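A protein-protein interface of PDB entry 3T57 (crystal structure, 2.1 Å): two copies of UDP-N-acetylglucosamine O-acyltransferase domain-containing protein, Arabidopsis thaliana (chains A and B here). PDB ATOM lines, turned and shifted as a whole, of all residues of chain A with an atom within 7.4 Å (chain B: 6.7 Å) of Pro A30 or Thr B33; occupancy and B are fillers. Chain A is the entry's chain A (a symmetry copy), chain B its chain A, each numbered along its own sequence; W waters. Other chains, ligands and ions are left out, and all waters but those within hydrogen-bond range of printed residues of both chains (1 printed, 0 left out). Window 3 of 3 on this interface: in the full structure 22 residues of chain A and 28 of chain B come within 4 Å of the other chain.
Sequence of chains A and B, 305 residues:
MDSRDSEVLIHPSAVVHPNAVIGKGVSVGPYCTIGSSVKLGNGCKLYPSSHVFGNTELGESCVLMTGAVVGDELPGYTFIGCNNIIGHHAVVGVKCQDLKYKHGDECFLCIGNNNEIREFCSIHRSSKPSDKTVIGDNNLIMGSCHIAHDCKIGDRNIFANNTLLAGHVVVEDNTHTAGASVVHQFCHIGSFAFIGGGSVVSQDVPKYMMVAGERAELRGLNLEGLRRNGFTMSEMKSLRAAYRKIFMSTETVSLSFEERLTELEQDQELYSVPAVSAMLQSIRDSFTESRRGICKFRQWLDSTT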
ATOM      1  N   ILE A  10      -4.584  27.713  -4.253  1.00  0.00           N
ATOM      2  CA  ILE A  10      -4.591  27.050  -2.966  1.00  0.00           C
ATOM      3  C   ILE A  10      -3.463  26.034  -2.945  1.00  0.00           C
ATOM      4  O   ILE A  10      -3.447  25.096  -3.747  1.00  0.00           O
ATOM      5  CB  ILE A  10      -5.954  26.357  -2.737  1.00  0.00           C
ATOM      6  CG1 ILE A  10      -7.096  27.383  -2.866  1.00  0.00           C
ATOM      7  CG2 ILE A  10      -5.975  25.648  -1.396  1.00  0.00           C
ATOM      8  CD1 ILE A  10      -8.519  26.759  -2.935  1.00  0.00           C
ATOM      9  N   HIS A  11      -2.507  26.232  -2.044  1.00  0.00           N
ATOM     10  CA  HIS A  11      -1.406  25.281  -1.893  1.00  0.00           C
ATOM     11  C   HIS A  11      -1.946  23.868  -1.589  1.00  0.00           C
ATOM     12  O   HIS A  11      -2.895  23.727  -0.805  1.00  0.00           O
ATOM     13  CB  HIS A  11      -0.437  25.734  -0.795  1.00  0.00           C
ATOM     14  CG  HIS A  11       0.889  25.047  -0.860  1.00  0.00           C
ATOM     15  ND1 HIS A  11       1.133  23.843  -0.236  1.00  0.00           N
ATOM     16  CD2 HIS A  11       2.028  25.371  -1.521  1.00  0.00           C
ATOM     17  CE1 HIS A  11       2.373  23.463  -0.494  1.00  0.00           C
ATOM     18  NE2 HIS A  11       2.935  24.372  -1.273  1.00  0.00           N
ATOM     19  N   PRO A  12      -1.368  22.823  -2.223  1.00  0.00           N
ATOM     20  CA  PRO A  12      -1.846  21.446  -1.990  1.00  0.00           C
ATOM     21  C   PRO A  12      -1.813  20.984  -0.525  1.00  0.00           C
ATOM     22  O   PRO A  12      -2.625  20.149  -0.143  1.00  0.00           O
ATOM     23  CB  PRO A  12      -0.901  20.577  -2.842  1.00  0.00           C
ATOM     24  CG  PRO A  12       0.220  21.489  -3.274  1.00  0.00           C
ATOM     25  CD  PRO A  12      -0.347  22.874  -3.290  1.00  0.00           C
ATOM     26  N   SER A  13      -0.901  21.527   0.283  1.00  0.00           N
ATOM     27  CA  SER A  13      -0.819  21.162   1.707  1.00  0.00           C
ATOM     28  C   SER A  13      -1.944  21.757   2.589  1.00  0.00           C
ATOM     29  O   SER A  13      -2.226  21.244   3.679  1.00  0.00           O
ATOM     30  CB  SER A  13       0.535  21.574   2.282  1.00  0.00           C
ATOM     31  OG  SER A  13       0.488  22.955   2.605  1.00  0.00           O
ATOM     32  N   ALA A  14      -2.583  22.826   2.138  1.00  0.00           N
ATOM     33  CA  ALA A  14      -3.623  23.487   2.937  1.00  0.00           C
ATOM     34  C   ALA A  14      -4.854  22.595   3.151  1.00  0.00           C
ATOM     35  O   ALA A  14      -5.209  21.792   2.283  1.00  0.00           O
ATOM     36  CB  ALA A  14      -4.021  24.798   2.291  1.00  0.00           C
ATOM     37  N   VAL A  15      -5.497  22.731   4.306  1.00  0.00           N
ATOM     38  CA  VAL A  15      -6.733  22.005   4.585  1.00  0.00           C
ATOM     39  C   VAL A  15      -7.899  22.977   4.412  1.00  0.00           C
ATOM     40  O   VAL A  15      -8.160  23.816   5.282  1.00  0.00           O
ATOM     41  CB  VAL A  15      -6.732  21.377   6.015  1.00  0.00           C
ATOM     42  CG1 VAL A  15      -8.065  20.663   6.313  1.00  0.00           C
ATOM     43  CG2 VAL A  15      -5.563  20.401   6.178  1.00  0.00           C
ATOM     44  N   VAL A  28      -4.299  30.896  -1.050  1.00  0.00           N
ATOM     45  CA  VAL A  28      -4.159  30.220   0.241  1.00  0.00           C
ATOM     46  C   VAL A  28      -2.802  29.508   0.318  1.00  0.00           C
ATOM     47  O   VAL A  28      -2.512  28.600  -0.475  1.00  0.00           O
ATOM     48  CB  VAL A  28      -5.322  29.221   0.497  1.00  0.00           C
ATOM     49  CG1 VAL A  28      -5.159  28.521   1.851  1.00  0.00           C
ATOM     50  CG2 VAL A  28      -6.661  29.937   0.451  1.00  0.00           C
ATOM     51  N   GLY A  29      -1.975  29.936   1.267  1.00  0.00           N
ATOM     52  CA  GLY A  29      -0.621  29.404   1.393  1.00  0.00           C
ATOM     53  C   GLY A  29      -0.547  28.042   2.067  1.00  0.00           C
ATOM     54  O   GLY A  29      -1.561  27.498   2.520  1.00  0.00           O
ATOM     55  N   PRO A  30       0.663  27.466   2.128  1.00  0.00           N
ATOM     56  CA  PRO A  30       0.812  26.162   2.770  1.00  0.00           C
ATOM     57  C   PRO A  30       0.423  26.146   4.250  1.00  0.00           C
ATOM     58  O   PRO A  30       0.636  27.126   4.965  1.00  0.00           O
ATOM     59  CB  PRO A  30       2.314  25.847   2.617  1.00  0.00           C
ATOM     60  CG  PRO A  30       2.969  27.148   2.214  1.00  0.00           C
ATOM     61  CD  PRO A  30       1.909  27.922   1.475  1.00  0.00           C
ATOM     62  N   TYR A  31      -0.144  25.020   4.687  1.00  0.00           N
ATOM     63  CA  TYR A  31      -0.490  24.766   6.105  1.00  0.00           C
ATOM     64  C   TYR A  31      -1.546  25.683   6.688  1.00  0.00           C
ATOM     65  O   TYR A  31      -1.635  25.818   7.915  1.00  0.00           O
ATOM     66  CB  TYR A  31       0.751  24.786   7.021  1.00  0.00           C
ATOM     67  CG  TYR A  31       1.956  24.147   6.389  1.00  0.00           C
ATOM     68  CD1 TYR A  31       1.925  22.815   5.961  1.00  0.00           C
ATOM     69  CD2 TYR A  31       3.122  24.879   6.205  1.00  0.00           C
ATOM     70  CE1 TYR A  31       3.048  22.243   5.354  1.00  0.00           C
ATOM     71  CE2 TYR A  31       4.221  24.327   5.611  1.00  0.00           C
ATOM     72  CZ  TYR A  31       4.184  23.020   5.192  1.00  0.00           C
ATOM     73  OH  TYR A  31       5.316  22.511   4.617  1.00  0.00           O
ATOM     74  N   CYS A  32      -2.343  26.306   5.827  1.00  0.00           N
ATOM     75  CA  CYS A  32      -3.528  27.024   6.290  1.00  0.00           C
ATOM     76  C   CYS A  32      -4.657  26.040   6.538  1.00  0.00           C
ATOM     77  O   CYS A  32      -4.686  24.962   5.955  1.00  0.00           O
ATOM     78  CB  CYS A  32      -3.994  28.053   5.251  1.00  0.00           C
ATOM     79  SG  CYS A  32      -2.815  29.371   4.937  1.00  0.00           S
ATOM     80  N   THR A  33      -5.598  26.424   7.397  1.00  0.00           N
ATOM     81  CA  THR A  33      -6.836  25.686   7.527  1.00  0.00           C
ATOM     82  C   THR A  33      -7.990  26.664   7.370  1.00  0.00           C
ATOM     83  O   THR A  33      -7.933  27.802   7.871  1.00  0.00           O
ATOM     84  CB  THR A  33      -6.931  24.920   8.865  1.00  0.00           C
ATOM     85  OG1 THR A  33      -6.984  25.858   9.951  1.00  0.00           O
ATOM     86  CG2 THR A  33      -5.701  24.013   9.044  1.00  0.00           C
ATOM     87  N   LEU A  46      -4.436  34.427   2.158  1.00  0.00           N
ATOM     88  CA  LEU A  46      -3.994  33.817   3.391  1.00  0.00           C
ATOM     89  C   LEU A  46      -2.522  33.410   3.262  1.00  0.00           C
ATOM     90  O   LEU A  46      -2.182  32.536   2.462  1.00  0.00           O
ATOM     91  CB  LEU A  46      -4.864  32.597   3.718  1.00  0.00           C
ATOM     92  CG  LEU A  46      -6.156  32.870   4.502  1.00  0.00           C
ATOM     93  CD1 LEU A  46      -7.163  33.713   3.705  1.00  0.00           C
ATOM     94  CD2 LEU A  46      -6.777  31.560   4.889  1.00  0.00           C
ATOM     95  N   TYR A  47      -1.661  34.048   4.054  1.00  0.00           N
ATOM     96  CA  TYR A  47      -0.238  33.677   4.107  1.00  0.00           C
ATOM     97  C   TYR A  47      -0.076  32.304   4.787  1.00  0.00           C
ATOM     98  O   TYR A  47      -1.055  31.775   5.321  1.00  0.00           O
ATOM     99  CB  TYR A  47       0.606  34.802   4.753  1.00  0.00           C
ATOM    100  CG  TYR A  47       0.897  35.922   3.770  1.00  0.00           C
ATOM    101  CD1 TYR A  47       2.091  35.947   3.034  1.00  0.00           C
ATOM    102  CD2 TYR A  47      -0.028  36.943   3.551  1.00  0.00           C
ATOM    103  CE1 TYR A  47       2.357  36.972   2.115  1.00  0.00           C
ATOM    104  CE2 TYR A  47       0.226  37.970   2.637  1.00  0.00           C
ATOM    105  CZ  TYR A  47       1.420  37.977   1.926  1.00  0.00           C
ATOM    106  OH  TYR A  47       1.656  38.991   1.020  1.00  0.00           O
ATOM    107  N   PRO A  48       1.131  31.695   4.714  1.00  0.00           N
ATOM    108  CA  PRO A  48       1.291  30.346   5.269  1.00  0.00           C
ATOM    109  C   PRO A  48       0.855  30.234   6.716  1.00  0.00           C
ATOM    110  O   PRO A  48       1.063  31.155   7.493  1.00  0.00           O
ATOM    111  CB  PRO A  48       2.800  30.091   5.137  1.00  0.00           C
ATOM    112  CG  PRO A  48       3.170  30.856   3.864  1.00  0.00           C
ATOM    113  CD  PRO A  48       2.317  32.110   3.926  1.00  0.00           C
ATOM    114  N   SER A  49       0.235  29.110   7.066  1.00  0.00           N
ATOM    115  CA  SER A  49      -0.155  28.831   8.453  1.00  0.00           C
ATOM    116  C   SER A  49      -1.067  29.891   9.064  1.00  0.00           C
ATOM    117  O   SER A  49      -0.887  30.289  10.220  1.00  0.00           O
ATOM    118  CB  SER A  49       1.084  28.632   9.331  1.00  0.00           C
ATOM    119  OG  SER A  49       2.040  27.873   8.622  1.00  0.00           O
ATOM    120  N   SER A  50      -2.040  30.347   8.284  1.00  0.00           N
ATOM    121  CA  SER A  50      -3.091  31.198   8.830  1.00  0.00           C
ATOM    122  C   SER A  50      -4.384  30.372   8.833  1.00  0.00           C
ATOM    123  O   SER A  50      -4.451  29.312   8.203  1.00  0.00           O
ATOM    124  CB  SER A  50      -3.211  32.528   8.056  1.00  0.00           C
ATOM    125  OG  SER A  50      -3.389  32.305   6.667  1.00  0.00           O
ATOM    126  N   THR A  66       0.902  35.280   8.461  1.00  0.00           N
ATOM    127  CA  THR A  66       1.221  33.995   9.089  1.00  0.00           C
ATOM    128  C   THR A  66       0.821  33.960  10.554  1.00  0.00           C
ATOM    129  O   THR A  66       1.085  34.899  11.321  1.00  0.00           O
ATOM    130  CB  THR A  66       2.711  33.647   8.910  1.00  0.00           C
ATOM    131  OG1 THR A  66       2.951  33.432   7.514  1.00  0.00           O
ATOM    132  CG2 THR A  66       3.101  32.389   9.687  1.00  0.00           C
ATOM    133  N   ALA B  14       8.194  20.150   5.220  1.00  0.00           N
ATOM    134  CA  ALA B  14       8.563  21.568   5.116  1.00  0.00           C
ATOM    135  C   ALA B  14       8.534  22.078   3.669  1.00  0.00           C
ATOM    136  O   ALA B  14       8.828  21.329   2.731  1.00  0.00           O
ATOM    137  CB  ALA B  14       9.926  21.797   5.735  1.00  0.00           C
ATOM    138  N   VAL B  15       8.174  23.343   3.488  1.00  0.00           N
ATOM    139  CA  VAL B  15       8.198  23.966   2.167  1.00  0.00           C
ATOM    140  C   VAL B  15       9.444  24.846   2.084  1.00  0.00           C
ATOM    141  O   VAL B  15       9.478  25.952   2.639  1.00  0.00           O
ATOM    142  CB  VAL B  15       6.904  24.795   1.886  1.00  0.00           C
ATOM    143  CG1 VAL B  15       6.973  25.488   0.513  1.00  0.00           C
ATOM    144  CG2 VAL B  15       5.661  23.903   1.966  1.00  0.00           C
ATOM    145  N   VAL B  16      10.480  24.324   1.437  1.00  0.00           N
ATOM    146  CA  VAL B  16      11.740  25.029   1.280  1.00  0.00           C
ATOM    147  C   VAL B  16      11.922  25.317  -0.207  1.00  0.00           C
ATOM    148  O   VAL B  16      12.088  24.392  -1.018  1.00  0.00           O
ATOM    149  CB  VAL B  16      12.933  24.202   1.807  1.00  0.00           C
ATOM    150  CG1 VAL B  16      14.250  24.962   1.619  1.00  0.00           C
ATOM    151  CG2 VAL B  16      12.727  23.814   3.277  1.00  0.00           C
ATOM    152  N   HIS B  17      11.852  26.594  -0.565  1.00  0.00           N
ATOM    153  CA  HIS B  17      11.950  26.982  -1.961  1.00  0.00           C
ATOM    154  C   HIS B  17      13.298  26.508  -2.519  1.00  0.00           C
ATOM    155  O   HIS B  17      14.312  26.597  -1.822  1.00  0.00           O
ATOM    156  CB  HIS B  17      11.810  28.499  -2.115  1.00  0.00           C
ATOM    157  CG  HIS B  17      11.587  28.933  -3.530  1.00  0.00           C
ATOM    158  ND1 HIS B  17      12.608  29.016  -4.453  1.00  0.00           N
ATOM    159  CD2 HIS B  17      10.453  29.278  -4.189  1.00  0.00           C
ATOM    160  CE1 HIS B  17      12.117  29.404  -5.616  1.00  0.00           C
ATOM    161  NE2 HIS B  17      10.815  29.575  -5.481  1.00  0.00           N
ATOM    162  N   VAL B  28      15.704  21.742   9.613  1.00  0.00           N
ATOM    163  CA  VAL B  28      14.404  22.371   9.372  1.00  0.00           C
ATOM    164  C   VAL B  28      13.274  21.411   9.761  1.00  0.00           C
ATOM    165  O   VAL B  28      13.136  20.321   9.185  1.00  0.00           O
ATOM    166  CB  VAL B  28      14.254  22.835   7.897  1.00  0.00           C
ATOM    167  CG1 VAL B  28      12.887  23.490   7.662  1.00  0.00           C
ATOM    168  CG2 VAL B  28      15.358  23.810   7.527  1.00  0.00           C
ATOM    169  N   GLY B  29      12.478  21.817  10.747  1.00  0.00           N
ATOM    170  CA  GLY B  29      11.419  20.962  11.272  1.00  0.00           C
ATOM    171  C   GLY B  29      10.169  20.914  10.404  1.00  0.00           C
ATOM    172  O   GLY B  29      10.071  21.611   9.386  1.00  0.00           O
ATOM    173  N   TYR B  31       6.541  21.512   8.781  1.00  0.00           N
ATOM    174  CA  TYR B  31       5.639  22.663   8.543  1.00  0.00           C
ATOM    175  C   TYR B  31       6.303  24.025   8.590  1.00  0.00           C
ATOM    176  O   TYR B  31       5.619  25.038   8.786  1.00  0.00           O
ATOM    177  CB  TYR B  31       4.429  22.663   9.500  1.00  0.00           C
ATOM    178  CG  TYR B  31       3.881  21.287   9.750  1.00  0.00           C
ATOM    179  CD1 TYR B  31       3.425  20.489   8.696  1.00  0.00           C
ATOM    180  CD2 TYR B  31       3.833  20.777  11.042  1.00  0.00           C
ATOM    181  CE1 TYR B  31       2.939  19.201   8.945  1.00  0.00           C
ATOM    182  CE2 TYR B  31       3.361  19.519  11.291  1.00  0.00           C
ATOM    183  CZ  TYR B  31       2.916  18.740  10.252  1.00  0.00           C
ATOM    184  OH  TYR B  31       2.439  17.495  10.557  1.00  0.00           O
ATOM    185  N   CYS B  32       7.619  24.059   8.409  1.00  0.00           N
ATOM    186  CA  CYS B  32       8.313  25.328   8.209  1.00  0.00           C
ATOM    187  C   CYS B  32       8.158  25.772   6.764  1.00  0.00           C
ATOM    188  O   CYS B  32       7.947  24.952   5.878  1.00  0.00           O
ATOM    189  CB  CYS B  32       9.809  25.199   8.523  1.00  0.00           C
ATOM    190  SG  CYS B  32      10.172  24.803  10.238  1.00  0.00           S
ATOM    191  N   THR B  33       8.283  27.076   6.530  1.00  0.00           N
ATOM    192  CA  THR B  33       8.399  27.584   5.181  1.00  0.00           C
ATOM    193  C   THR B  33       9.632  28.473   5.112  1.00  0.00           C
ATOM    194  O   THR B  33       9.917  29.239   6.052  1.00  0.00           O
ATOM    195  CB  THR B  33       7.136  28.347   4.723  1.00  0.00           C
ATOM    196  OG1 THR B  33       6.980  29.533   5.516  1.00  0.00           O
ATOM    197  CG2 THR B  33       5.891  27.458   4.897  1.00  0.00           C
ATOM    198  N   ILE B  34      10.368  28.333   4.013  1.00  0.00           N
ATOM    199  CA  ILE B  34      11.565  29.121   3.743  1.00  0.00           C
ATOM    200  C   ILE B  34      11.452  29.620   2.304  1.00  0.00           C
ATOM    201  O   ILE B  34      11.300  28.821   1.368  1.00  0.00           O
ATOM    202  CB  ILE B  34      12.871  28.297   3.910  1.00  0.00           C
ATOM    203  CG1 ILE B  34      12.988  27.723   5.329  1.00  0.00           C
ATOM    204  CG2 ILE B  34      14.099  29.178   3.584  1.00  0.00           C
ATOM    205  CD1 ILE B  34      14.153  26.726   5.530  1.00  0.00           C
ATOM    206  N   GLY B  35      11.493  30.941   2.147  1.00  0.00           N
ATOM    207  CA  GLY B  35      11.266  31.582   0.861  1.00  0.00           C
ATOM    208  C   GLY B  35      12.470  31.488  -0.065  1.00  0.00           C
ATOM    209  O   GLY B  35      13.551  31.035   0.325  1.00  0.00           O
ATOM    210  N   VAL B  38      15.966  33.578   0.807  1.00  0.00           N
ATOM    211  CA  VAL B  38      16.494  33.440   2.151  1.00  0.00           C
ATOM    212  C   VAL B  38      17.865  32.751   2.082  1.00  0.00           C
ATOM    213  O   VAL B  38      18.058  31.795   1.310  1.00  0.00           O
ATOM    214  CB  VAL B  38      15.532  32.596   3.046  1.00  0.00           C
ATOM    215  CG1 VAL B  38      16.142  32.328   4.424  1.00  0.00           C
ATOM    216  CG2 VAL B  38      14.164  33.271   3.192  1.00  0.00           C
ATOM    217  N   LEU B  46      15.662  25.521  12.527  1.00  0.00           N
ATOM    218  CA  LEU B  46      14.286  25.965  12.529  1.00  0.00           C
ATOM    219  C   LEU B  46      13.406  24.901  13.193  1.00  0.00           C
ATOM    220  O   LEU B  46      13.266  23.791  12.673  1.00  0.00           O
ATOM    221  CB  LEU B  46      13.818  26.236  11.095  1.00  0.00           C
ATOM    222  CG  LEU B  46      14.104  27.637  10.536  1.00  0.00           C
ATOM    223  CD1 LEU B  46      15.606  27.918  10.384  1.00  0.00           C
ATOM    224  CD2 LEU B  46      13.420  27.781   9.208  1.00  0.00           C
ATOM    225  N   SER B  49       7.102  24.597  12.344  1.00  0.00           N
ATOM    226  CA  SER B  49       6.228  25.740  12.056  1.00  0.00           C
ATOM    227  C   SER B  49       6.883  27.096  12.307  1.00  0.00           C
ATOM    228  O   SER B  49       6.259  28.004  12.866  1.00  0.00           O
ATOM    229  CB  SER B  49       4.920  25.632  12.845  1.00  0.00           C
ATOM    230  OG  SER B  49       4.479  24.291  12.832  1.00  0.00           O
ATOM    231  N   SER B  50       8.138  27.226  11.896  1.00  0.00           N
ATOM    232  CA  SER B  50       8.786  28.532  11.893  1.00  0.00           C
ATOM    233  C   SER B  50       8.963  28.944  10.425  1.00  0.00           C
ATOM    234  O   SER B  50       8.812  28.117   9.521  1.00  0.00           O
ATOM    235  CB  SER B  50      10.105  28.520  12.693  1.00  0.00           C
ATOM    236  OG  SER B  50      10.980  27.502  12.235  1.00  0.00           O
ATOM    237  N   HIS B  51       9.208  30.226  10.186  1.00  0.00           N
ATOM    238  CA  HIS B  51       9.061  30.786   8.837  1.00  0.00           C
ATOM    239  C   HIS B  51      10.105  31.863   8.549  1.00  0.00           C
ATOM    240  O   HIS B  51      10.355  32.726   9.395  1.00  0.00           O
ATOM    241  CB  HIS B  51       7.664  31.397   8.678  1.00  0.00           C
ATOM    242  CG  HIS B  51       6.550  30.472   9.073  1.00  0.00           C
ATOM    243  ND1 HIS B  51       5.925  29.632   8.173  1.00  0.00           N
ATOM    244  CD2 HIS B  51       5.947  30.259  10.269  1.00  0.00           C
ATOM    245  CE1 HIS B  51       5.004  28.924   8.804  1.00  0.00           C
ATOM    246  NE2 HIS B  51       4.990  29.291  10.075  1.00  0.00           N
ATOM    247  N   VAL B  52      10.698  31.823   7.353  1.00  0.00           N
ATOM    248  CA  VAL B  52      11.573  32.900   6.903  1.00  0.00           C
ATOM    249  C   VAL B  52      11.092  33.366   5.534  1.00  0.00           C
ATOM    250  O   VAL B  52      10.962  32.551   4.609  1.00  0.00           O
ATOM    251  CB  VAL B  52      13.073  32.466   6.832  1.00  0.00           C
ATOM    252  CG1 VAL B  52      13.956  33.697   6.762  1.00  0.00           C
ATOM    253  CG2 VAL B  52      13.464  31.594   8.048  1.00  0.00           C
ATOM    254  N   PHE B  53      10.816  34.666   5.416  1.00  0.00           N
ATOM    255  CA  PHE B  53      10.272  35.272   4.187  1.00  0.00           C
ATOM    256  C   PHE B  53      11.218  36.349   3.647  1.00  0.00           C
ATOM    257  O   PHE B  53      12.099  36.849   4.366  1.00  0.00           O
ATOM    258  CB  PHE B  53       8.923  35.967   4.450  1.00  0.00           C
ATOM    259  CG  PHE B  53       7.806  35.045   4.893  1.00  0.00           C
ATOM    260  CD1 PHE B  53       7.095  34.289   3.960  1.00  0.00           C
ATOM    261  CD2 PHE B  53       7.450  34.956   6.241  1.00  0.00           C
ATOM    262  CE1 PHE B  53       6.044  33.434   4.376  1.00  0.00           C
ATOM    263  CE2 PHE B  53       6.396  34.123   6.666  1.00  0.00           C
ATOM    264  CZ  PHE B  53       5.704  33.357   5.741  1.00  0.00           C
HETATM  265  O   HOH W   1       3.310  26.021   9.770  1.00  0.00           O
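Among the printed residues, pairs that only touch across the chains: Pro A30 with Val B15 (3.9 Å), Pro A30 with Thr B33 (3.98 Å), Tyr A31 with Ala B14 (3.4 Å), Tyr A31 with Tyr B31 (3.5 Å), Tyr A31 with Cys B32 (3.8 Å), Tyr A31 with Thr B33 (3.6 Å), Pro A48 with Phe B53 (3.9 Å), Ser A49 with His B51 (3.2 Å), Thr A66 with His B51 (3.6 Å) and Thr A66 with Phe B53 (3.3 Å).
Water W1 bridges the side-chain hydroxyl of Ser A49 and the backbone carbonyl oxygen of Tyr B31.
SG of Cys A32 is in hydrogen-bond range of N of Ser A49 (3.7 Å).
N of Tyr A31 is in hydrogen-bond range of OG of Ser A13 (3.0 Å).
The backbone carbonyl oxygen (O) of Cys B32 lies within hydrogen-bond range of the backbone NH (N) of Val B15 (2.9 Å).
The backbone carbonyl oxygen (O) of Pro A48 is in hydrogen-bond range of the side-chain hydroxyl (OG1) of Thr A66, at 3.0 Å.
O of Gly B29 lies within hydrogen-bond range of SG of Cys B32 (3.3 Å).
The backbone carbonyl oxygen (O) of Thr B33 sits at hydrogen-bond distance from the backbone NH (N) of Val B52.
OH of Tyr A31 sits close to N of Val B15 (3.2 Å).
Printed residues of chain A that touch a printed residue of chain B: Pro A30, Tyr A31, Pro A48, Ser A49 and Thr A66.
Among the printed residues, 11 pairs touch across the chains.
Among the printed residues, no Asp or Glu carboxylate lies within 4 Å of a Lys or Arg side-chain nitrogen of the other chain.
Pro A30 touches two residues of chain B.
Thr B33 touches two residues of chain A.
Of the printed residues of chain A, His B51 touches Ser A49 (3.2 Å) and Thr A66 (3.6 Å).
Of the printed residues of chain A, Ala B14 touches Tyr A31.
Of the printed residues of chain B, Thr A66 touches His B51 (3.6 Å) and Phe B53 (3.3 Å).
The nearest printed residue of chain A that does not touch Tyr B31 is Ser A49 (4.6 Å).
Tyr A31 touches Val B15, but with the chains exchanged Val A15 does not touch Tyr B31 (9.0 Å).
Tyr A31 touches its own counterpart, Tyr B31.
Tyr A31 touches Cys B32, but with the chains exchanged Cys A32 does not touch Tyr B31 (8.5 Å).
Tyr A31 touches Thr B33, but with the chains exchanged Thr A33 does not touch Tyr B31 (9.8 Å).
10 positions are printed for both chains.
Of the 11 pairs that touch across the chains among the printed residues, 1 has its exchanged pair printed and touching as well.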
